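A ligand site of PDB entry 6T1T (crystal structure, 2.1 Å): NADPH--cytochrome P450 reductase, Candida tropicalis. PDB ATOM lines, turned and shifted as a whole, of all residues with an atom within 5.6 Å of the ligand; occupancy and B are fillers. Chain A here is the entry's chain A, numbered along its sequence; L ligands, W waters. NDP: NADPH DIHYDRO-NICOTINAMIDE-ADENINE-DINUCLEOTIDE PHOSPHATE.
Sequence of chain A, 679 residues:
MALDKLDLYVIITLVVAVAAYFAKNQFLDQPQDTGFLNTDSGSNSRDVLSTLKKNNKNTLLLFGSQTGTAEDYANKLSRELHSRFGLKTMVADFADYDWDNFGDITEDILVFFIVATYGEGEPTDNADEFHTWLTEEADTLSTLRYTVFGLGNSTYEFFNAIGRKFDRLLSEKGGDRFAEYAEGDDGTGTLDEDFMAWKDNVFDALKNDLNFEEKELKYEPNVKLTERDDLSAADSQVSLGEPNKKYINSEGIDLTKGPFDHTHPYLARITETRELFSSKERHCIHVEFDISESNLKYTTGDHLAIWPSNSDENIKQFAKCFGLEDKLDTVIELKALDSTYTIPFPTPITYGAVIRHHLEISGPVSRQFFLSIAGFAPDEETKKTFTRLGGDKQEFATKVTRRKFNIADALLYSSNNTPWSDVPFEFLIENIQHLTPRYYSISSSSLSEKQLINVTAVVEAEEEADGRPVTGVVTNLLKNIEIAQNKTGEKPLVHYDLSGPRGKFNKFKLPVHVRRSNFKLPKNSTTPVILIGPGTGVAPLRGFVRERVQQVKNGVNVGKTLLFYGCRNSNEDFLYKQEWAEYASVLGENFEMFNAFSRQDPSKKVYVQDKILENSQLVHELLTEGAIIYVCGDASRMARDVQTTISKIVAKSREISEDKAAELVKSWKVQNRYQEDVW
OG1 of Thr 536 is in hydrogen-bond range of O1N of the ligand.
OG of Ser 598 sits at hydrogen-bond distance from O2B of the ligand, 2.6 Å away.
An oxygen (O3X) of the ligand lies within salt-bridge range of the guanidinium group (NE) of Arg 599.
The side-chain hydroxyl (OH) of Tyr 607 sits at hydrogen-bond distance from an oxygen (O2X) of the ligand, 2.6 Å away.
The side-chain amino group (NZ) of Lys 605 is in salt-bridge range of an oxygen (O3X) of the ligand, 2.7 Å away.
An oxygen (O2A) of the ligand is in salt-bridge range of the guanidinium group (NH2) of Arg 282.
O of Cys 567 sits close to O3B of the ligand (3.3 Å).
A nitrogen (N1A) of the ligand is in hydrogen-bond range of the side-chain amide nitrogen (NE2) of Gln 609 (3.2 Å).
The backbone NH (N) of Thr 536 lies within hydrogen-bond range of an oxygen (O1N) of the ligand (2.9 Å).
The side-chain carboxylate of Asp 641 lies within hydrogen-bond range of a nitrogen (N6A) of the ligand (3.0 Å).
The backbone NH (N) of Arg 568 sits at hydrogen-bond distance from an oxygen (O3B) of the ligand (3.4 Å).
O of Arg 568 is in hydrogen-bond range of N of Arg 599 (2.7 Å).
The side-chain carboxylate (OD2) of Asp 634 is in hydrogen-bond range of the backbone NH (N) of Arg 637, at 2.9 Å.
The guanidinium group of Arg 282 is in salt-bridge range of the side-chain carboxylate of Asp 573, at 3.3 Å.
The side-chain carboxylate (OD2) of Asp 641 sits close to the side-chain amide nitrogen (NE2) of Gln 609 (3.4 Å).
The backbone NH (N) of Cys 567 sits at hydrogen-bond distance from the backbone carbonyl oxygen (O) of Ala 596, at 3.1 Å.
The side-chain sulfur (SG) of Cys 567 lies within hydrogen-bond range of the side-chain carboxylate (OD1) of Asp 573, 3.6 Å away.
OD2 of Asp 634 is in hydrogen-bond range of N of Met 638, 3.1 Å away.
The backbone NH (N) of Ser 598 is in hydrogen-bond range of the backbone carbonyl oxygen (O) of Arg 568 (3.4 Å).
A nitrogen (N6A) of the ligand sits close to the backbone NH of Met 638, 3.3 Å away.
CG1 of Val 458 touches O2N of the ligand, at 3.9 Å.
Pro 534 touches the ligand (CB to O4B, 3.8 Å).
Gly 535 touches the ligand.
Arg 637 touches the ligand (CB to N6A, 3.3 Å).
Hydrophobic or aromatic side chains that line the ligand: Val 458, Pro 534, Tyr 607 and Met 638.
Within 4 Å of the ligand: Arg 282, Val 458, Pro 534, Gly 535, Thr 536, Cys 567, Arg 568, Ser 598, Arg 599, Lys 605, Tyr 607, Gln 609, Arg 637, Met 638 and Asp 641.
Water W3 bridges N3A of the ligand and N of Val 608.
Water W2 lies within hydrogen-bond range of the backbone carbonyl oxygen (O) of Ala 596, an oxygen (O3B) of the ligand and the backbone NH (N) of Cys 567.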
ATOM      1  N   ARG A 282      25.886 -24.559 -37.417  1.00  0.00           N
ATOM      2  CA  ARG A 282      24.575 -25.255 -37.281  1.00  0.00           C
ATOM      3  C   ARG A 282      23.702 -24.852 -38.474  1.00  0.00           C
ATOM      4  O   ARG A 282      23.745 -23.660 -38.818  1.00  0.00           O
ATOM      5  CB  ARG A 282      23.936 -24.847 -35.947  1.00  0.00           C
ATOM      6  CG  ARG A 282      22.958 -25.844 -35.355  1.00  0.00           C
ATOM      7  CD  ARG A 282      22.628 -25.514 -33.913  1.00  0.00           C
ATOM      8  NE  ARG A 282      21.261 -25.932 -33.646  1.00  0.00           N
ATOM      9  CZ  ARG A 282      20.229 -25.120 -33.456  1.00  0.00           C
ATOM     10  NH1 ARG A 282      20.368 -23.808 -33.422  1.00  0.00           N
ATOM     11  NH2 ARG A 282      19.029 -25.638 -33.261  1.00  0.00           N
ATOM     12  N   VAL A 458      16.657 -29.766 -39.983  1.00  0.00           N
ATOM     13  CA  VAL A 458      17.867 -29.288 -39.257  1.00  0.00           C
ATOM     14  C   VAL A 458      18.968 -30.326 -39.493  1.00  0.00           C
ATOM     15  O   VAL A 458      18.696 -31.537 -39.391  1.00  0.00           O
ATOM     16  CB  VAL A 458      17.613 -28.983 -37.768  1.00  0.00           C
ATOM     17  CG1 VAL A 458      17.046 -30.173 -37.019  1.00  0.00           C
ATOM     18  CG2 VAL A 458      18.855 -28.464 -37.054  1.00  0.00           C
ATOM     19  N   PRO A 534       8.655 -25.658 -30.582  1.00  0.00           N
ATOM     20  CA  PRO A 534       9.930 -24.975 -30.667  1.00  0.00           C
ATOM     21  C   PRO A 534      10.859 -25.729 -31.634  1.00  0.00           C
ATOM     22  O   PRO A 534      10.655 -26.949 -31.858  1.00  0.00           O
ATOM     23  CB  PRO A 534      10.512 -25.052 -29.261  1.00  0.00           C
ATOM     24  CG  PRO A 534       9.890 -26.307 -28.678  1.00  0.00           C
ATOM     25  CD  PRO A 534       8.538 -26.452 -29.350  1.00  0.00           C
ATOM     26  N   GLY A 535      11.868 -25.007 -32.123  1.00  0.00           N
ATOM     27  CA  GLY A 535      12.806 -25.472 -33.172  1.00  0.00           C
ATOM     28  C   GLY A 535      12.053 -25.968 -34.388  1.00  0.00           C
ATOM     29  O   GLY A 535      11.107 -25.324 -34.813  1.00  0.00           O
ATOM     30  N   THR A 536      12.438 -27.118 -34.916  1.00  0.00           N
ATOM     31  CA  THR A 536      11.847 -27.703 -36.142  1.00  0.00           C
ATOM     32  C   THR A 536      10.454 -28.281 -35.812  1.00  0.00           C
ATOM     33  O   THR A 536       9.748 -28.672 -36.761  1.00  0.00           O
ATOM     34  CB  THR A 536      12.824 -28.716 -36.754  1.00  0.00           C
ATOM     35  OG1 THR A 536      13.164 -29.650 -35.732  1.00  0.00           O
ATOM     36  CG2 THR A 536      14.083 -28.067 -37.266  1.00  0.00           C
ATOM     37  N   GLY A 537      10.055 -28.296 -34.536  1.00  0.00           N
ATOM     38  CA  GLY A 537       8.648 -28.546 -34.152  1.00  0.00           C
ATOM     39  C   GLY A 537       7.694 -27.591 -34.873  1.00  0.00           C
ATOM     40  O   GLY A 537       6.535 -27.984 -35.124  1.00  0.00           O
ATOM     41  N   GLY A 566       9.729 -21.417 -29.945  1.00  0.00           N
ATOM     42  CA  GLY A 566      10.996 -21.262 -29.232  1.00  0.00           C
ATOM     43  C   GLY A 566      12.157 -21.489 -30.182  1.00  0.00           C
ATOM     44  O   GLY A 566      12.003 -22.256 -31.144  1.00  0.00           O
ATOM     45  N   CYS A 567      13.267 -20.809 -29.927  1.00  0.00           N
ATOM     46  CA  CYS A 567      14.564 -20.947 -30.619  1.00  0.00           C
ATOM     47  C   CYS A 567      15.643 -20.329 -29.710  1.00  0.00           C
ATOM     48  O   CYS A 567      15.284 -19.727 -28.701  1.00  0.00           O
ATOM     49  CB  CYS A 567      14.507 -20.330 -32.009  1.00  0.00           C
ATOM     50  SG  CYS A 567      14.578 -18.523 -32.017  1.00  0.00           S
ATOM     51  N   ARG A 568      16.915 -20.590 -29.981  1.00  0.00           N
ATOM     52  CA  ARG A 568      18.024 -20.075 -29.131  1.00  0.00           C
ATOM     53  C   ARG A 568      17.997 -18.547 -29.088  1.00  0.00           C
ATOM     54  O   ARG A 568      18.130 -17.972 -27.988  1.00  0.00           O
ATOM     55  CB  ARG A 568      19.370 -20.520 -29.691  1.00  0.00           C
ATOM     56  CG  ARG A 568      19.599 -22.015 -29.579  1.00  0.00           C
ATOM     57  CD  ARG A 568      20.794 -22.291 -30.450  1.00  0.00           C
ATOM     58  NE  ARG A 568      21.209 -23.670 -30.342  1.00  0.00           N
ATOM     59  CZ  ARG A 568      22.424 -24.098 -30.634  1.00  0.00           C
ATOM     60  NH1 ARG A 568      23.343 -23.243 -31.043  1.00  0.00           N
ATOM     61  NH2 ARG A 568      22.707 -25.381 -30.484  1.00  0.00           N
ATOM     62  N   ASP A 573      18.460 -18.496 -35.136  1.00  0.00           N
ATOM     63  CA  ASP A 573      17.787 -19.746 -35.564  1.00  0.00           C
ATOM     64  C   ASP A 573      16.270 -19.611 -35.512  1.00  0.00           C
ATOM     65  O   ASP A 573      15.603 -20.636 -35.333  1.00  0.00           O
ATOM     66  CB  ASP A 573      18.253 -20.921 -34.704  1.00  0.00           C
ATOM     67  CG  ASP A 573      18.124 -20.629 -33.213  1.00  0.00           C
ATOM     68  OD1 ASP A 573      17.954 -19.445 -32.885  1.00  0.00           O
ATOM     69  OD2 ASP A 573      18.184 -21.595 -32.410  1.00  0.00           O
ATOM     70  N   ALA A 596       9.856 -18.000 -27.303  1.00  0.00           N
ATOM     71  CA  ALA A 596      10.790 -18.200 -26.176  1.00  0.00           C
ATOM     72  C   ALA A 596      12.232 -18.311 -26.719  1.00  0.00           C
ATOM     73  O   ALA A 596      12.607 -19.395 -27.241  1.00  0.00           O
ATOM     74  CB  ALA A 596      10.364 -19.412 -25.386  1.00  0.00           C
ATOM     75  N   SER A 598      15.674 -19.026 -25.960  1.00  0.00           N
ATOM     76  CA  SER A 598      16.273 -19.807 -24.850  1.00  0.00           C
ATOM     77  C   SER A 598      17.685 -19.321 -24.494  1.00  0.00           C
ATOM     78  O   SER A 598      18.200 -19.761 -23.428  1.00  0.00           O
ATOM     79  CB  SER A 598      16.288 -21.292 -25.163  1.00  0.00           C
ATOM     80  OG  SER A 598      17.005 -21.582 -26.351  1.00  0.00           O
ATOM     81  N   ARG A 599      18.338 -18.516 -25.330  1.00  0.00           N
ATOM     82  CA  ARG A 599      19.752 -18.081 -25.093  1.00  0.00           C
ATOM     83  C   ARG A 599      19.915 -16.574 -25.239  1.00  0.00           C
ATOM     84  O   ARG A 599      21.003 -16.132 -24.935  1.00  0.00           O
ATOM     85  CB  ARG A 599      20.709 -18.837 -26.025  1.00  0.00           C
ATOM     86  CG  ARG A 599      20.512 -20.345 -25.943  1.00  0.00           C
ATOM     87  CD  ARG A 599      21.679 -21.113 -26.469  1.00  0.00           C
ATOM     88  NE  ARG A 599      21.360 -22.529 -26.543  1.00  0.00           N
ATOM     89  CZ  ARG A 599      22.160 -23.447 -27.069  1.00  0.00           C
ATOM     90  NH1 ARG A 599      23.326 -23.098 -27.581  1.00  0.00           N
ATOM     91  NH2 ARG A 599      21.788 -24.715 -27.104  1.00  0.00           N
ATOM     92  N   LYS A 605      17.436 -19.517 -19.093  1.00  0.00           N
ATOM     93  CA  LYS A 605      16.672 -20.208 -20.174  1.00  0.00           C
ATOM     94  C   LYS A 605      15.195 -19.810 -20.116  1.00  0.00           C
ATOM     95  O   LYS A 605      14.653 -19.688 -19.015  1.00  0.00           O
ATOM     96  CB  LYS A 605      16.764 -21.738 -20.057  1.00  0.00           C
ATOM     97  CG  LYS A 605      18.153 -22.326 -20.200  1.00  0.00           C
ATOM     98  CD  LYS A 605      18.505 -22.823 -21.600  1.00  0.00           C
ATOM     99  CE  LYS A 605      20.000 -23.023 -21.765  1.00  0.00           C
ATOM    100  NZ  LYS A 605      20.361 -23.354 -23.163  1.00  0.00           N
ATOM    101  N   TYR A 607      11.659 -21.081 -22.239  1.00  0.00           N
ATOM    102  CA  TYR A 607      11.067 -22.078 -23.166  1.00  0.00           C
ATOM    103  C   TYR A 607       9.581 -21.805 -23.372  1.00  0.00           C
ATOM    104  O   TYR A 607       8.932 -21.014 -22.600  1.00  0.00           O
ATOM    105  CB  TYR A 607      11.261 -23.487 -22.589  1.00  0.00           C
ATOM    106  CG  TYR A 607      12.689 -23.926 -22.466  1.00  0.00           C
ATOM    107  CD1 TYR A 607      13.645 -23.556 -23.394  1.00  0.00           C
ATOM    108  CD2 TYR A 607      13.085 -24.782 -21.445  1.00  0.00           C
ATOM    109  CE1 TYR A 607      14.950 -23.988 -23.305  1.00  0.00           C
ATOM    110  CE2 TYR A 607      14.395 -25.220 -21.325  1.00  0.00           C
ATOM    111  CZ  TYR A 607      15.333 -24.827 -22.271  1.00  0.00           C
ATOM    112  OH  TYR A 607      16.625 -25.234 -22.181  1.00  0.00           O
ATOM    113  N   VAL A 608       9.008 -22.484 -24.376  1.00  0.00           N
ATOM    114  CA  VAL A 608       7.557 -22.381 -24.667  1.00  0.00           C
ATOM    115  C   VAL A 608       6.755 -22.551 -23.351  1.00  0.00           C
ATOM    116  O   VAL A 608       5.866 -21.714 -23.084  1.00  0.00           O
ATOM    117  CB  VAL A 608       7.113 -23.374 -25.764  1.00  0.00           C
ATOM    118  CG1 VAL A 608       7.789 -23.079 -27.103  1.00  0.00           C
ATOM    119  CG2 VAL A 608       7.302 -24.829 -25.347  1.00  0.00           C
ATOM    120  N   GLN A 609       7.070 -23.574 -22.521  1.00  0.00           N
ATOM    121  CA  GLN A 609       6.259 -23.850 -21.296  1.00  0.00           C
ATOM    122  C   GLN A 609       6.199 -22.585 -20.413  1.00  0.00           C
ATOM    123  O   GLN A 609       5.114 -22.320 -19.868  1.00  0.00           O
ATOM    124  CB  GLN A 609       6.766 -25.072 -20.523  1.00  0.00           C
ATOM    125  CG  GLN A 609       8.251 -25.053 -20.201  1.00  0.00           C
ATOM    126  CD  GLN A 609       9.052 -25.776 -21.263  1.00  0.00           C
ATOM    127  OE1 GLN A 609       8.905 -25.535 -22.471  1.00  0.00           O
ATOM    128  NE2 GLN A 609       9.905 -26.681 -20.791  1.00  0.00           N
ATOM    129  N   ASP A 634      10.697 -31.890 -30.268  1.00  0.00           N
ATOM    130  CA  ASP A 634      11.540 -32.757 -29.394  1.00  0.00           C
ATOM    131  C   ASP A 634      10.635 -33.620 -28.502  1.00  0.00           C
ATOM    132  O   ASP A 634       9.979 -33.079 -27.601  1.00  0.00           O
ATOM    133  CB  ASP A 634      12.470 -31.913 -28.512  1.00  0.00           C
ATOM    134  CG  ASP A 634      13.232 -32.756 -27.497  1.00  0.00           C
ATOM    135  OD1 ASP A 634      13.896 -33.694 -27.927  1.00  0.00           O
ATOM    136  OD2 ASP A 634      13.134 -32.486 -26.281  1.00  0.00           O
ATOM    137  N   ARG A 637      12.353 -34.319 -24.177  1.00  0.00           N
ATOM    138  CA  ARG A 637      12.312 -33.389 -23.008  1.00  0.00           C
ATOM    139  C   ARG A 637      11.141 -32.402 -23.133  1.00  0.00           C
ATOM    140  O   ARG A 637      10.266 -32.436 -22.267  1.00  0.00           O
ATOM    141  CB  ARG A 637      13.610 -32.613 -22.870  1.00  0.00           C
ATOM    142  CG  ARG A 637      14.807 -33.458 -22.476  1.00  0.00           C
ATOM    143  CD  ARG A 637      16.066 -32.621 -22.356  1.00  0.00           C
ATOM    144  NE  ARG A 637      16.993 -33.157 -21.369  1.00  0.00           N
ATOM    145  CZ  ARG A 637      16.805 -33.149 -20.043  1.00  0.00           C
ATOM    146  NH1 ARG A 637      15.711 -32.623 -19.521  1.00  0.00           N
ATOM    147  NH2 ARG A 637      17.721 -33.669 -19.232  1.00  0.00           N
ATOM    148  N   MET A 638      11.138 -31.550 -24.156  1.00  0.00           N
ATOM    149  CA  MET A 638      10.098 -30.530 -24.367  1.00  0.00           C
ATOM    150  C   MET A 638       8.691 -31.149 -24.246  1.00  0.00           C
ATOM    151  O   MET A 638       7.912 -30.631 -23.437  1.00  0.00           O
ATOM    152  CB  MET A 638      10.269 -29.855 -25.724  1.00  0.00           C
ATOM    153  CG  MET A 638       9.228 -28.799 -26.042  1.00  0.00           C
ATOM    154  SD  MET A 638       7.726 -29.446 -26.887  1.00  0.00           S
ATOM    155  CE  MET A 638       8.401 -30.045 -28.428  1.00  0.00           C
ATOM    156  N   ASP A 641       7.732 -31.824 -20.590  1.00  0.00           N
ATOM    157  CA  ASP A 641       7.710 -30.508 -19.908  1.00  0.00           C
ATOM    158  C   ASP A 641       6.424 -29.768 -20.260  1.00  0.00           C
ATOM    159  O   ASP A 641       5.803 -29.233 -19.336  1.00  0.00           O
ATOM    160  CB  ASP A 641       8.925 -29.655 -20.274  1.00  0.00           C
ATOM    161  CG  ASP A 641      10.158 -30.168 -19.591  1.00  0.00           C
ATOM    162  OD1 ASP A 641      10.001 -31.045 -18.734  1.00  0.00           O
ATOM    163  OD2 ASP A 641      11.235 -29.689 -19.908  1.00  0.00           O
HETATM  164  PA  NDP L   1      16.682 -27.228 -30.731  1.00  0.00           P
HETATM  165  O1A NDP L   1      16.726 -28.530 -30.015  1.00  0.00           O
HETATM  166  O2A NDP L   1      17.711 -26.166 -30.463  1.00  0.00           O
HETATM  167  O5B NDP L   1      15.247 -26.577 -30.542  1.00  0.00           O
HETATM  168  C5B NDP L   1      14.813 -26.606 -29.215  1.00  0.00           C
HETATM  169  C4B NDP L   1      14.563 -25.205 -28.724  1.00  0.00           C
HETATM  170  O4B NDP L   1      13.820 -25.396 -27.503  1.00  0.00           O
HETATM  171  C3B NDP L   1      15.778 -24.369 -28.303  1.00  0.00           C
HETATM  172  O3B NDP L   1      15.529 -22.992 -28.078  1.00  0.00           O
HETATM  173  C2B NDP L   1      16.109 -25.053 -26.983  1.00  0.00           C
HETATM  174  O2B NDP L   1      16.792 -24.131 -26.173  1.00  0.00           O
HETATM  175  C1B NDP L   1      14.706 -25.274 -26.416  1.00  0.00           C
HETATM  176  N9A NDP L   1      14.574 -26.427 -25.538  1.00  0.00           N
HETATM  177  C8A NDP L   1      15.553 -27.302 -25.120  1.00  0.00           C
HETATM  178  N7A NDP L   1      15.115 -28.170 -24.237  1.00  0.00           N
HETATM  179  C5A NDP L   1      13.778 -27.829 -24.041  1.00  0.00           C
HETATM  180  C6A NDP L   1      12.762 -28.380 -23.225  1.00  0.00           C
HETATM  181  N6A NDP L   1      12.936 -29.406 -22.402  1.00  0.00           N
HETATM  182  N1A NDP L   1      11.544 -27.798 -23.278  1.00  0.00           N
HETATM  183  C2A NDP L   1      11.359 -26.770 -24.109  1.00  0.00           C
HETATM  184  N3A NDP L   1      12.232 -26.168 -24.916  1.00  0.00           N
HETATM  185  C4A NDP L   1      13.434 -26.752 -24.838  1.00  0.00           C
HETATM  186  O3  NDP L   1      16.558 -27.517 -32.316  1.00  0.00           O
HETATM  187  PN  NDP L   1      15.799 -28.750 -32.973  1.00  0.00           P
HETATM  188  O1N NDP L   1      14.948 -28.313 -34.112  1.00  0.00           O
HETATM  189  O2N NDP L   1      16.831 -29.803 -33.160  1.00  0.00           O
HETATM  190  O5D NDP L   1      14.818 -29.182 -31.764  1.00  0.00           O
HETATM  191  P2B NDP L   1      18.232 -24.601 -25.638  1.00  0.00           P
HETATM  192  O1X NDP L   1      18.849 -25.495 -26.711  1.00  0.00           O
HETATM  193  O2X NDP L   1      18.058 -25.339 -24.356  1.00  0.00           O
HETATM  194  O3X NDP L   1      18.965 -23.270 -25.449  1.00  0.00           O
HETATM  195  O   HOH W   1      12.801 -28.414 -28.016  1.00  0.00           O
HETATM  196  O   HOH W   2      12.991 -21.760 -26.730  1.00  0.00           O
HETATM  197  O   HOH W   3      11.198 -23.794 -26.088  1.00  0.00           O
